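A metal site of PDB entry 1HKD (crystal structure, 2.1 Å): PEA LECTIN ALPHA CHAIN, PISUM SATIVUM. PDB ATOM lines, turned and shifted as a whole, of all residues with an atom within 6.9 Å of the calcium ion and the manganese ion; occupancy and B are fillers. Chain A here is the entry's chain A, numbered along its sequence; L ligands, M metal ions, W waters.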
ATOM      1  N   ASP A  81      21.299 -29.518   7.877  1.00  0.00           N
ATOM      2  CA  ASP A  81      21.242 -28.060   7.864  1.00  0.00           C
ATOM      3  C   ASP A  81      22.531 -27.512   8.468  1.00  0.00           C
ATOM      4  O   ASP A  81      22.962 -26.390   8.224  1.00  0.00           O
ATOM      5  CB  ASP A  81      20.111 -27.631   8.768  1.00  0.00           C
ATOM      6  CG  ASP A  81      18.831 -27.543   8.031  1.00  0.00           C
ATOM      7  OD1 ASP A  81      17.961 -28.414   8.240  1.00  0.00           O
ATOM      8  OD2 ASP A  81      18.622 -26.654   7.192  1.00  0.00           O
ATOM      9  N   GLY A  82      22.994 -28.314   9.496  1.00  0.00           N
ATOM     10  CA  GLY A  82      24.245 -27.896  10.113  1.00  0.00           C
ATOM     11  C   GLY A  82      24.373 -28.350  11.546  1.00  0.00           C
ATOM     12  O   GLY A  82      23.565 -29.140  12.055  1.00  0.00           O
ATOM     13  N   GLY A  98      15.274 -27.996  11.618  1.00  0.00           N
ATOM     14  CA  GLY A  98      15.600 -27.541  10.283  1.00  0.00           C
ATOM     15  C   GLY A  98      16.690 -26.472  10.290  1.00  0.00           C
ATOM     16  O   GLY A  98      17.702 -26.599  10.996  1.00  0.00           O
ATOM     17  N   GLY A  99      16.466 -25.406   9.504  1.00  0.00           N
ATOM     18  CA  GLY A  99      17.401 -24.291   9.393  1.00  0.00           C
ATOM     19  C   GLY A  99      17.633 -23.508  10.692  1.00  0.00           C
ATOM     20  O   GLY A  99      18.546 -22.687  10.762  1.00  0.00           O
ATOM     21  N   TYR A 100      16.790 -23.755  11.692  1.00  0.00           N
ATOM     22  CA  TYR A 100      16.923 -23.104  12.986  1.00  0.00           C
ATOM     23  C   TYR A 100      17.919 -23.849  13.886  1.00  0.00           C
ATOM     24  O   TYR A 100      18.190 -23.431  15.011  1.00  0.00           O
ATOM     25  CB  TYR A 100      15.549 -22.964  13.667  1.00  0.00           C
ATOM     26  CG  TYR A 100      14.634 -22.008  12.941  1.00  0.00           C
ATOM     27  CD1 TYR A 100      14.746 -20.636  13.130  1.00  0.00           C
ATOM     28  CD2 TYR A 100      13.730 -22.468  11.993  1.00  0.00           C
ATOM     29  CE1 TYR A 100      13.903 -19.743  12.441  1.00  0.00           C
ATOM     30  CE2 TYR A 100      12.902 -21.605  11.307  1.00  0.00           C
ATOM     31  CZ  TYR A 100      12.993 -20.246  11.535  1.00  0.00           C
ATOM     32  OH  TYR A 100      12.151 -19.409  10.854  1.00  0.00           O
ATOM     33  N   LEU A 101      18.416 -24.978  13.388  1.00  0.00           N
ATOM     34  CA  LEU A 101      19.477 -25.761  14.056  1.00  0.00           C
ATOM     35  C   LEU A 101      19.201 -26.219  15.469  1.00  0.00           C
ATOM     36  O   LEU A 101      20.149 -26.518  16.217  1.00  0.00           O
ATOM     37  CB  LEU A 101      20.815 -25.013  13.992  1.00  0.00           C
ATOM     38  CG  LEU A 101      21.174 -24.470  12.600  1.00  0.00           C
ATOM     39  CD1 LEU A 101      22.421 -23.577  12.645  1.00  0.00           C
ATOM     40  CD2 LEU A 101      21.365 -25.619  11.611  1.00  0.00           C
ATOM     41  N   GLU A 119      27.563 -21.422  14.774  1.00  0.00           N
ATOM     42  CA  GLU A 119      27.009 -22.340  13.802  1.00  0.00           C
ATOM     43  C   GLU A 119      27.968 -22.698  12.684  1.00  0.00           C
ATOM     44  O   GLU A 119      28.834 -21.924  12.319  1.00  0.00           O
ATOM     45  CB  GLU A 119      25.718 -21.752  13.205  1.00  0.00           C
ATOM     46  CG  GLU A 119      25.925 -20.425  12.491  1.00  0.00           C
ATOM     47  CD  GLU A 119      24.722 -20.005  11.680  1.00  0.00           C
ATOM     48  OE1 GLU A 119      24.884 -19.707  10.487  1.00  0.00           O
ATOM     49  OE2 GLU A 119      23.596 -20.037  12.225  1.00  0.00           O
ATOM     50  N   PHE A 120      27.778 -23.903  12.149  1.00  0.00           N
ATOM     51  CA  PHE A 120      28.506 -24.396  10.984  1.00  0.00           C
ATOM     52  C   PHE A 120      27.351 -24.778  10.080  1.00  0.00           C
ATOM     53  O   PHE A 120      26.793 -25.867  10.186  1.00  0.00           O
ATOM     54  CB  PHE A 120      29.367 -25.590  11.383  1.00  0.00           C
ATOM     55  CG  PHE A 120      30.395 -25.251  12.454  1.00  0.00           C
ATOM     56  CD1 PHE A 120      30.046 -25.297  13.799  1.00  0.00           C
ATOM     57  CD2 PHE A 120      31.637 -24.751  12.101  1.00  0.00           C
ATOM     58  CE1 PHE A 120      30.948 -24.917  14.788  1.00  0.00           C
ATOM     59  CE2 PHE A 120      32.551 -24.358  13.087  1.00  0.00           C
ATOM     60  CZ  PHE A 120      32.205 -24.455  14.433  1.00  0.00           C
ATOM     61  N   ASP A 121      26.913 -23.795   9.311  1.00  0.00           N
ATOM     62  CA  ASP A 121      25.733 -23.853   8.466  1.00  0.00           C
ATOM     63  C   ASP A 121      26.010 -24.392   7.061  1.00  0.00           C
ATOM     64  O   ASP A 121      26.716 -23.758   6.291  1.00  0.00           O
ATOM     65  CB  ASP A 121      25.134 -22.445   8.386  1.00  0.00           C
ATOM     66  CG  ASP A 121      23.692 -22.432   7.951  1.00  0.00           C
ATOM     67  OD1 ASP A 121      23.234 -23.384   7.261  1.00  0.00           O
ATOM     68  OD2 ASP A 121      22.948 -21.471   8.250  1.00  0.00           O
ATOM     69  N   THR A 122      25.359 -25.503   6.707  1.00  0.00           N
ATOM     70  CA  THR A 122      25.584 -26.121   5.401  1.00  0.00           C
ATOM     71  C   THR A 122      24.487 -25.880   4.372  1.00  0.00           C
ATOM     72  O   THR A 122      24.602 -26.354   3.233  1.00  0.00           O
ATOM     73  CB  THR A 122      25.741 -27.658   5.552  1.00  0.00           C
ATOM     74  OG1 THR A 122      24.629 -28.172   6.305  1.00  0.00           O
ATOM     75  CG2 THR A 122      26.975 -28.009   6.366  1.00  0.00           C
ATOM     76  N   PHE A 123      23.408 -25.224   4.775  1.00  0.00           N
ATOM     77  CA  PHE A 123      22.287 -25.005   3.865  1.00  0.00           C
ATOM     78  C   PHE A 123      21.814 -23.565   3.871  1.00  0.00           C
ATOM     79  O   PHE A 123      21.477 -23.016   4.918  1.00  0.00           O
ATOM     80  CB  PHE A 123      21.122 -25.964   4.215  1.00  0.00           C
ATOM     81  CG  PHE A 123      19.919 -25.832   3.320  1.00  0.00           C
ATOM     82  CD1 PHE A 123      18.915 -24.930   3.612  1.00  0.00           C
ATOM     83  CD2 PHE A 123      19.760 -26.668   2.212  1.00  0.00           C
ATOM     84  CE1 PHE A 123      17.804 -24.786   2.785  1.00  0.00           C
ATOM     85  CE2 PHE A 123      18.646 -26.546   1.381  1.00  0.00           C
ATOM     86  CZ  PHE A 123      17.678 -25.606   1.667  1.00  0.00           C
ATOM     87  N   TYR A 124      21.764 -22.984   2.675  1.00  0.00           N
ATOM     88  CA  TYR A 124      21.320 -21.617   2.470  1.00  0.00           C
ATOM     89  C   TYR A 124      19.801 -21.434   2.647  1.00  0.00           C
ATOM     90  O   TYR A 124      19.018 -21.899   1.819  1.00  0.00           O
ATOM     91  CB  TYR A 124      21.730 -21.142   1.059  1.00  0.00           C
ATOM     92  CG  TYR A 124      21.119 -19.814   0.634  1.00  0.00           C
ATOM     93  CD1 TYR A 124      21.468 -18.631   1.270  1.00  0.00           C
ATOM     94  CD2 TYR A 124      20.167 -19.760  -0.391  1.00  0.00           C
ATOM     95  CE1 TYR A 124      20.913 -17.411   0.896  1.00  0.00           C
ATOM     96  CE2 TYR A 124      19.603 -18.535  -0.786  1.00  0.00           C
ATOM     97  CZ  TYR A 124      19.990 -17.369  -0.135  1.00  0.00           C
ATOM     98  OH  TYR A 124      19.443 -16.156  -0.500  1.00  0.00           O
ATOM     99  N   ASN A 125      19.404 -20.742   3.717  1.00  0.00           N
ATOM    100  CA  ASN A 125      18.008 -20.400   3.960  1.00  0.00           C
ATOM    101  C   ASN A 125      17.838 -18.958   3.501  1.00  0.00           C
ATOM    102  O   ASN A 125      18.370 -18.047   4.131  1.00  0.00           O
ATOM    103  CB  ASN A 125      17.668 -20.526   5.446  1.00  0.00           C
ATOM    104  CG  ASN A 125      17.699 -21.955   5.948  1.00  0.00           C
ATOM    105  OD1 ASN A 125      18.731 -22.446   6.379  1.00  0.00           O
ATOM    106  ND2 ASN A 125      16.545 -22.619   5.931  1.00  0.00           N
ATOM    107  N   TRP A 128      17.230 -15.537   5.728  1.00  0.00           N
ATOM    108  CA  TRP A 128      18.195 -14.930   6.652  1.00  0.00           C
ATOM    109  C   TRP A 128      19.694 -15.180   6.400  1.00  0.00           C
ATOM    110  O   TRP A 128      20.529 -14.420   6.889  1.00  0.00           O
ATOM    111  CB  TRP A 128      17.849 -15.307   8.105  1.00  0.00           C
ATOM    112  CG  TRP A 128      17.963 -16.790   8.377  1.00  0.00           C
ATOM    113  CD1 TRP A 128      19.113 -17.515   8.477  1.00  0.00           C
ATOM    114  CD2 TRP A 128      16.892 -17.725   8.457  1.00  0.00           C
ATOM    115  NE1 TRP A 128      18.824 -18.854   8.665  1.00  0.00           N
ATOM    116  CE2 TRP A 128      17.459 -19.009   8.661  1.00  0.00           C
ATOM    117  CE3 TRP A 128      15.503 -17.621   8.428  1.00  0.00           C
ATOM    118  CZ2 TRP A 128      16.691 -20.157   8.802  1.00  0.00           C
ATOM    119  CZ3 TRP A 128      14.736 -18.761   8.575  1.00  0.00           C
ATOM    120  CH2 TRP A 128      15.337 -20.020   8.739  1.00  0.00           C
ATOM    121  N   ASP A 129      20.042 -16.221   5.642  1.00  0.00           N
ATOM    122  CA  ASP A 129      21.464 -16.523   5.406  1.00  0.00           C
ATOM    123  C   ASP A 129      22.131 -15.587   4.406  1.00  0.00           C
ATOM    124  O   ASP A 129      21.457 -14.994   3.565  1.00  0.00           O
ATOM    125  CB  ASP A 129      21.623 -17.972   4.965  1.00  0.00           C
ATOM    126  CG  ASP A 129      21.567 -18.948   6.123  1.00  0.00           C
ATOM    127  OD1 ASP A 129      21.971 -18.585   7.247  1.00  0.00           O
ATOM    128  OD2 ASP A 129      21.168 -20.129   5.968  1.00  0.00           O
ATOM    129  N   PRO A 130      23.464 -15.516   4.445  1.00  0.00           N
ATOM    130  CA  PRO A 130      24.231 -14.654   3.524  1.00  0.00           C
ATOM    131  C   PRO A 130      23.814 -14.885   2.073  1.00  0.00           C
ATOM    132  O   PRO A 130      23.825 -16.027   1.617  1.00  0.00           O
ATOM    133  CB  PRO A 130      25.672 -15.109   3.763  1.00  0.00           C
ATOM    134  CG  PRO A 130      25.679 -15.560   5.197  1.00  0.00           C
ATOM    135  CD  PRO A 130      24.359 -16.261   5.347  1.00  0.00           C
ATOM    136  N   HIS A 136      28.726 -21.600   5.633  1.00  0.00           N
ATOM    137  CA  HIS A 136      29.460 -20.627   6.428  1.00  0.00           C
ATOM    138  C   HIS A 136      29.478 -20.929   7.897  1.00  0.00           C
ATOM    139  O   HIS A 136      28.672 -21.705   8.405  1.00  0.00           O
ATOM    140  CB  HIS A 136      28.795 -19.254   6.241  1.00  0.00           C
ATOM    141  CG  HIS A 136      27.307 -19.273   6.448  1.00  0.00           C
ATOM    142  ND1 HIS A 136      26.428 -19.779   5.507  1.00  0.00           N
ATOM    143  CD2 HIS A 136      26.547 -18.940   7.530  1.00  0.00           C
ATOM    144  CE1 HIS A 136      25.202 -19.734   5.985  1.00  0.00           C
ATOM    145  NE2 HIS A 136      25.243 -19.232   7.209  1.00  0.00           N
ATOM    146  N   ILE A 137      30.445 -20.303   8.575  1.00  0.00           N
ATOM    147  CA  ILE A 137      30.540 -20.352  10.026  1.00  0.00           C
ATOM    148  C   ILE A 137      29.895 -19.048  10.486  1.00  0.00           C
ATOM    149  O   ILE A 137      30.040 -18.021   9.833  1.00  0.00           O
ATOM    150  CB  ILE A 137      32.019 -20.390  10.472  1.00  0.00           C
ATOM    151  CG1 ILE A 137      32.724 -21.621   9.885  1.00  0.00           C
ATOM    152  CG2 ILE A 137      32.126 -20.422  11.998  1.00  0.00           C
ATOM    153  CD1 ILE A 137      34.258 -21.555  10.027  1.00  0.00           C
ATOM    154  N   GLY A 138      29.141 -19.104  11.584  1.00  0.00           N
ATOM    155  CA  GLY A 138      28.481 -17.911  12.061  1.00  0.00           C
ATOM    156  C   GLY A 138      28.392 -17.825  13.566  1.00  0.00           C
ATOM    157  O   GLY A 138      28.494 -18.827  14.274  1.00  0.00           O
ATOM    158  N   ASP A 140      25.920 -16.602  16.460  1.00  0.00           N
ATOM    159  CA  ASP A 140      24.510 -16.290  16.629  1.00  0.00           C
ATOM    160  C   ASP A 140      24.214 -15.814  18.037  1.00  0.00           C
ATOM    161  O   ASP A 140      24.641 -16.437  19.017  1.00  0.00           O
ATOM    162  CB  ASP A 140      23.659 -17.527  16.313  1.00  0.00           C
ATOM    163  CG  ASP A 140      23.848 -18.041  14.892  1.00  0.00           C
ATOM    164  OD1 ASP A 140      24.385 -17.309  14.040  1.00  0.00           O
ATOM    165  OD2 ASP A 140      23.455 -19.181  14.544  1.00  0.00           O
ATOM    166  N   ILE A 144      18.717 -16.683  14.697  1.00  0.00           N
ATOM    167  CA  ILE A 144      19.300 -17.560  13.673  1.00  0.00           C
ATOM    168  C   ILE A 144      20.061 -16.747  12.618  1.00  0.00           C
ATOM    169  O   ILE A 144      20.834 -17.282  11.824  1.00  0.00           O
ATOM    170  CB  ILE A 144      18.234 -18.462  13.032  1.00  0.00           C
ATOM    171  CG1 ILE A 144      18.885 -19.645  12.289  1.00  0.00           C
ATOM    172  CG2 ILE A 144      17.313 -17.684  12.090  1.00  0.00           C
ATOM    173  CD1 ILE A 144      19.760 -20.532  13.185  1.00  0.00           C
ATOM    174  N   LYS A 145      19.821 -15.443  12.611  1.00  0.00           N
ATOM    175  CA  LYS A 145      20.510 -14.566  11.669  1.00  0.00           C
ATOM    176  C   LYS A 145      21.781 -14.075  12.353  1.00  0.00           C
ATOM    177  O   LYS A 145      21.717 -13.241  13.251  1.00  0.00           O
ATOM    178  CB  LYS A 145      19.616 -13.385  11.294  1.00  0.00           C
ATOM    179  CG  LYS A 145      20.224 -12.432  10.263  1.00  0.00           C
ATOM    180  CD  LYS A 145      19.254 -11.294   9.961  1.00  0.00           C
ATOM    181  CE  LYS A 145      19.915 -10.182   9.163  1.00  0.00           C
ATOM    182  NZ  LYS A 145      18.951  -9.069   8.843  1.00  0.00           N
ATOM    183  N   SER A 146      22.928 -14.607  11.923  1.00  0.00           N
ATOM    184  CA  SER A 146      24.211 -14.315  12.552  1.00  0.00           C
ATOM    185  C   SER A 146      24.631 -12.843  12.598  1.00  0.00           C
ATOM    186  O   SER A 146      24.315 -12.070  11.701  1.00  0.00           O
ATOM    187  CB  SER A 146      25.326 -15.146  11.888  1.00  0.00           C
ATOM    188  OG  SER A 146      24.914 -16.493  11.672  1.00  0.00           O
ATOM    189  N   THR A 149      29.569 -13.698   9.888  1.00  0.00           N
ATOM    190  CA  THR A 149      29.760 -14.994   9.251  1.00  0.00           C
ATOM    191  C   THR A 149      31.067 -15.031   8.477  1.00  0.00           C
ATOM    192  O   THR A 149      31.689 -13.988   8.219  1.00  0.00           O
ATOM    193  CB  THR A 149      28.616 -15.298   8.256  1.00  0.00           C
ATOM    194  OG1 THR A 149      28.496 -14.214   7.307  1.00  0.00           O
ATOM    195  CG2 THR A 149      27.266 -15.347   8.950  1.00  0.00           C
HETATM  196  C1  LIG L   1      13.228 -27.087   4.478  1.00  0.00           C
HETATM  197  C2  LIG L   1      13.061 -26.554   5.903  1.00  0.00           C
HETATM  198  C3  LIG L   1      14.229 -25.648   6.284  1.00  0.00           C
HETATM  199  C4  LIG L   1      15.550 -26.382   6.059  1.00  0.00           C
HETATM  200  C5  LIG L   1      15.618 -26.969   4.659  1.00  0.00           C
HETATM  201  C6  LIG L   1      16.874 -27.805   4.465  1.00  0.00           C
HETATM  202  C7  LIG L   1      13.129 -26.493   2.158  1.00  0.00           C
HETATM  203  O1  LIG L   1      13.157 -26.012   3.515  1.00  0.00           O
HETATM  204  O2  LIG L   1      11.831 -25.825   6.034  1.00  0.00           O
HETATM  205  O3  LIG L   1      14.102 -25.264   7.666  1.00  0.00           O
HETATM  206  O4  LIG L   1      16.612 -25.437   6.222  1.00  0.00           O
HETATM  207  O5  LIG L   1      14.473 -27.785   4.371  1.00  0.00           O
HETATM  208  O6  LIG L   1      16.776 -29.001   5.235  1.00  0.00           O
HETATM  209 CA    CA M   1      20.991 -22.317   7.026  1.00  0.00          CA
HETATM  210 MN    MN M   2      23.462 -19.262   8.755  1.00  0.00          MN
HETATM  211  O   HOH W   1      23.883 -17.136   9.339  1.00  0.00           O
HETATM  212  O   HOH W   2      20.350 -21.639   9.191  1.00  0.00           O
HETATM  213  O   HOH W   3      21.869 -19.323  10.458  1.00  0.00           O
HETATM  214  O   HOH W   4      20.722 -24.584   7.584  1.00  0.00           O
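The backbone carbonyl oxygen (O) of Phe 123 binds the calcium ion (2.3 Å).
The calcium ion is bound by water W4, 2.4 Å away.
The calcium ion is bound by OD1 of Asn 125, 2.4 Å away.
Water W2 binds the calcium ion (2.4 Å).
OD2 of Asp 129 is bound to the calcium ion (2.4 Å).
The calcium ion is bound by OD2 of Asp 121 (2.5 Å).
OD1 of Asp 121 binds the calcium ion.
Water W2 bridges O of Gly 99 (2.6 Å) and NE1 of Trp 128 (3.2 Å).
Water W3 bridges OE2 of Glu 119 (2.6 Å) and O of Ile 144 (2.7 Å).
The manganese ion is bound by OD1 of Asp 129, water W1, OE1 of Glu 119, OD2 of Asp 121, water W3 and NE2 of His 136.
The manganese ion has six donor atoms within binding distance.
The side-chain carboxylate (OD2) of Asp 140 lies close to the side-chain carboxylate (OE2) of Glu 119, at 2.5 Å.
The side-chain carboxylate (OD1) of Asp 129 sits close to the indole nitrogen (NE1) of Trp 128 (3.5 Å).
The backbone NH (N) of Glu 119 is in hydrogen-bond range of the backbone carbonyl oxygen (O) of Gly 138 (2.8 Å).
OE1 of Glu 119 sits close to OG of Ser 146, 3.4 Å away.
Of the 24 residues printed, 4 come within 4 Å of the manganese ion.
The nearest printed residue that does not touch the manganese ion is Ser 146 (4.3 Å).
The backbone NH (N) of Gly 99 is in hydrogen-bond range of an oxygen (O3) of the ligand, at 3.0 Å.
ND2 of Asn 125 sits at hydrogen-bond distance from O4 of the ligand (2.8 Å).
OD2 of Asp 81 is in hydrogen-bond range of O4 of the ligand (2.5 Å).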
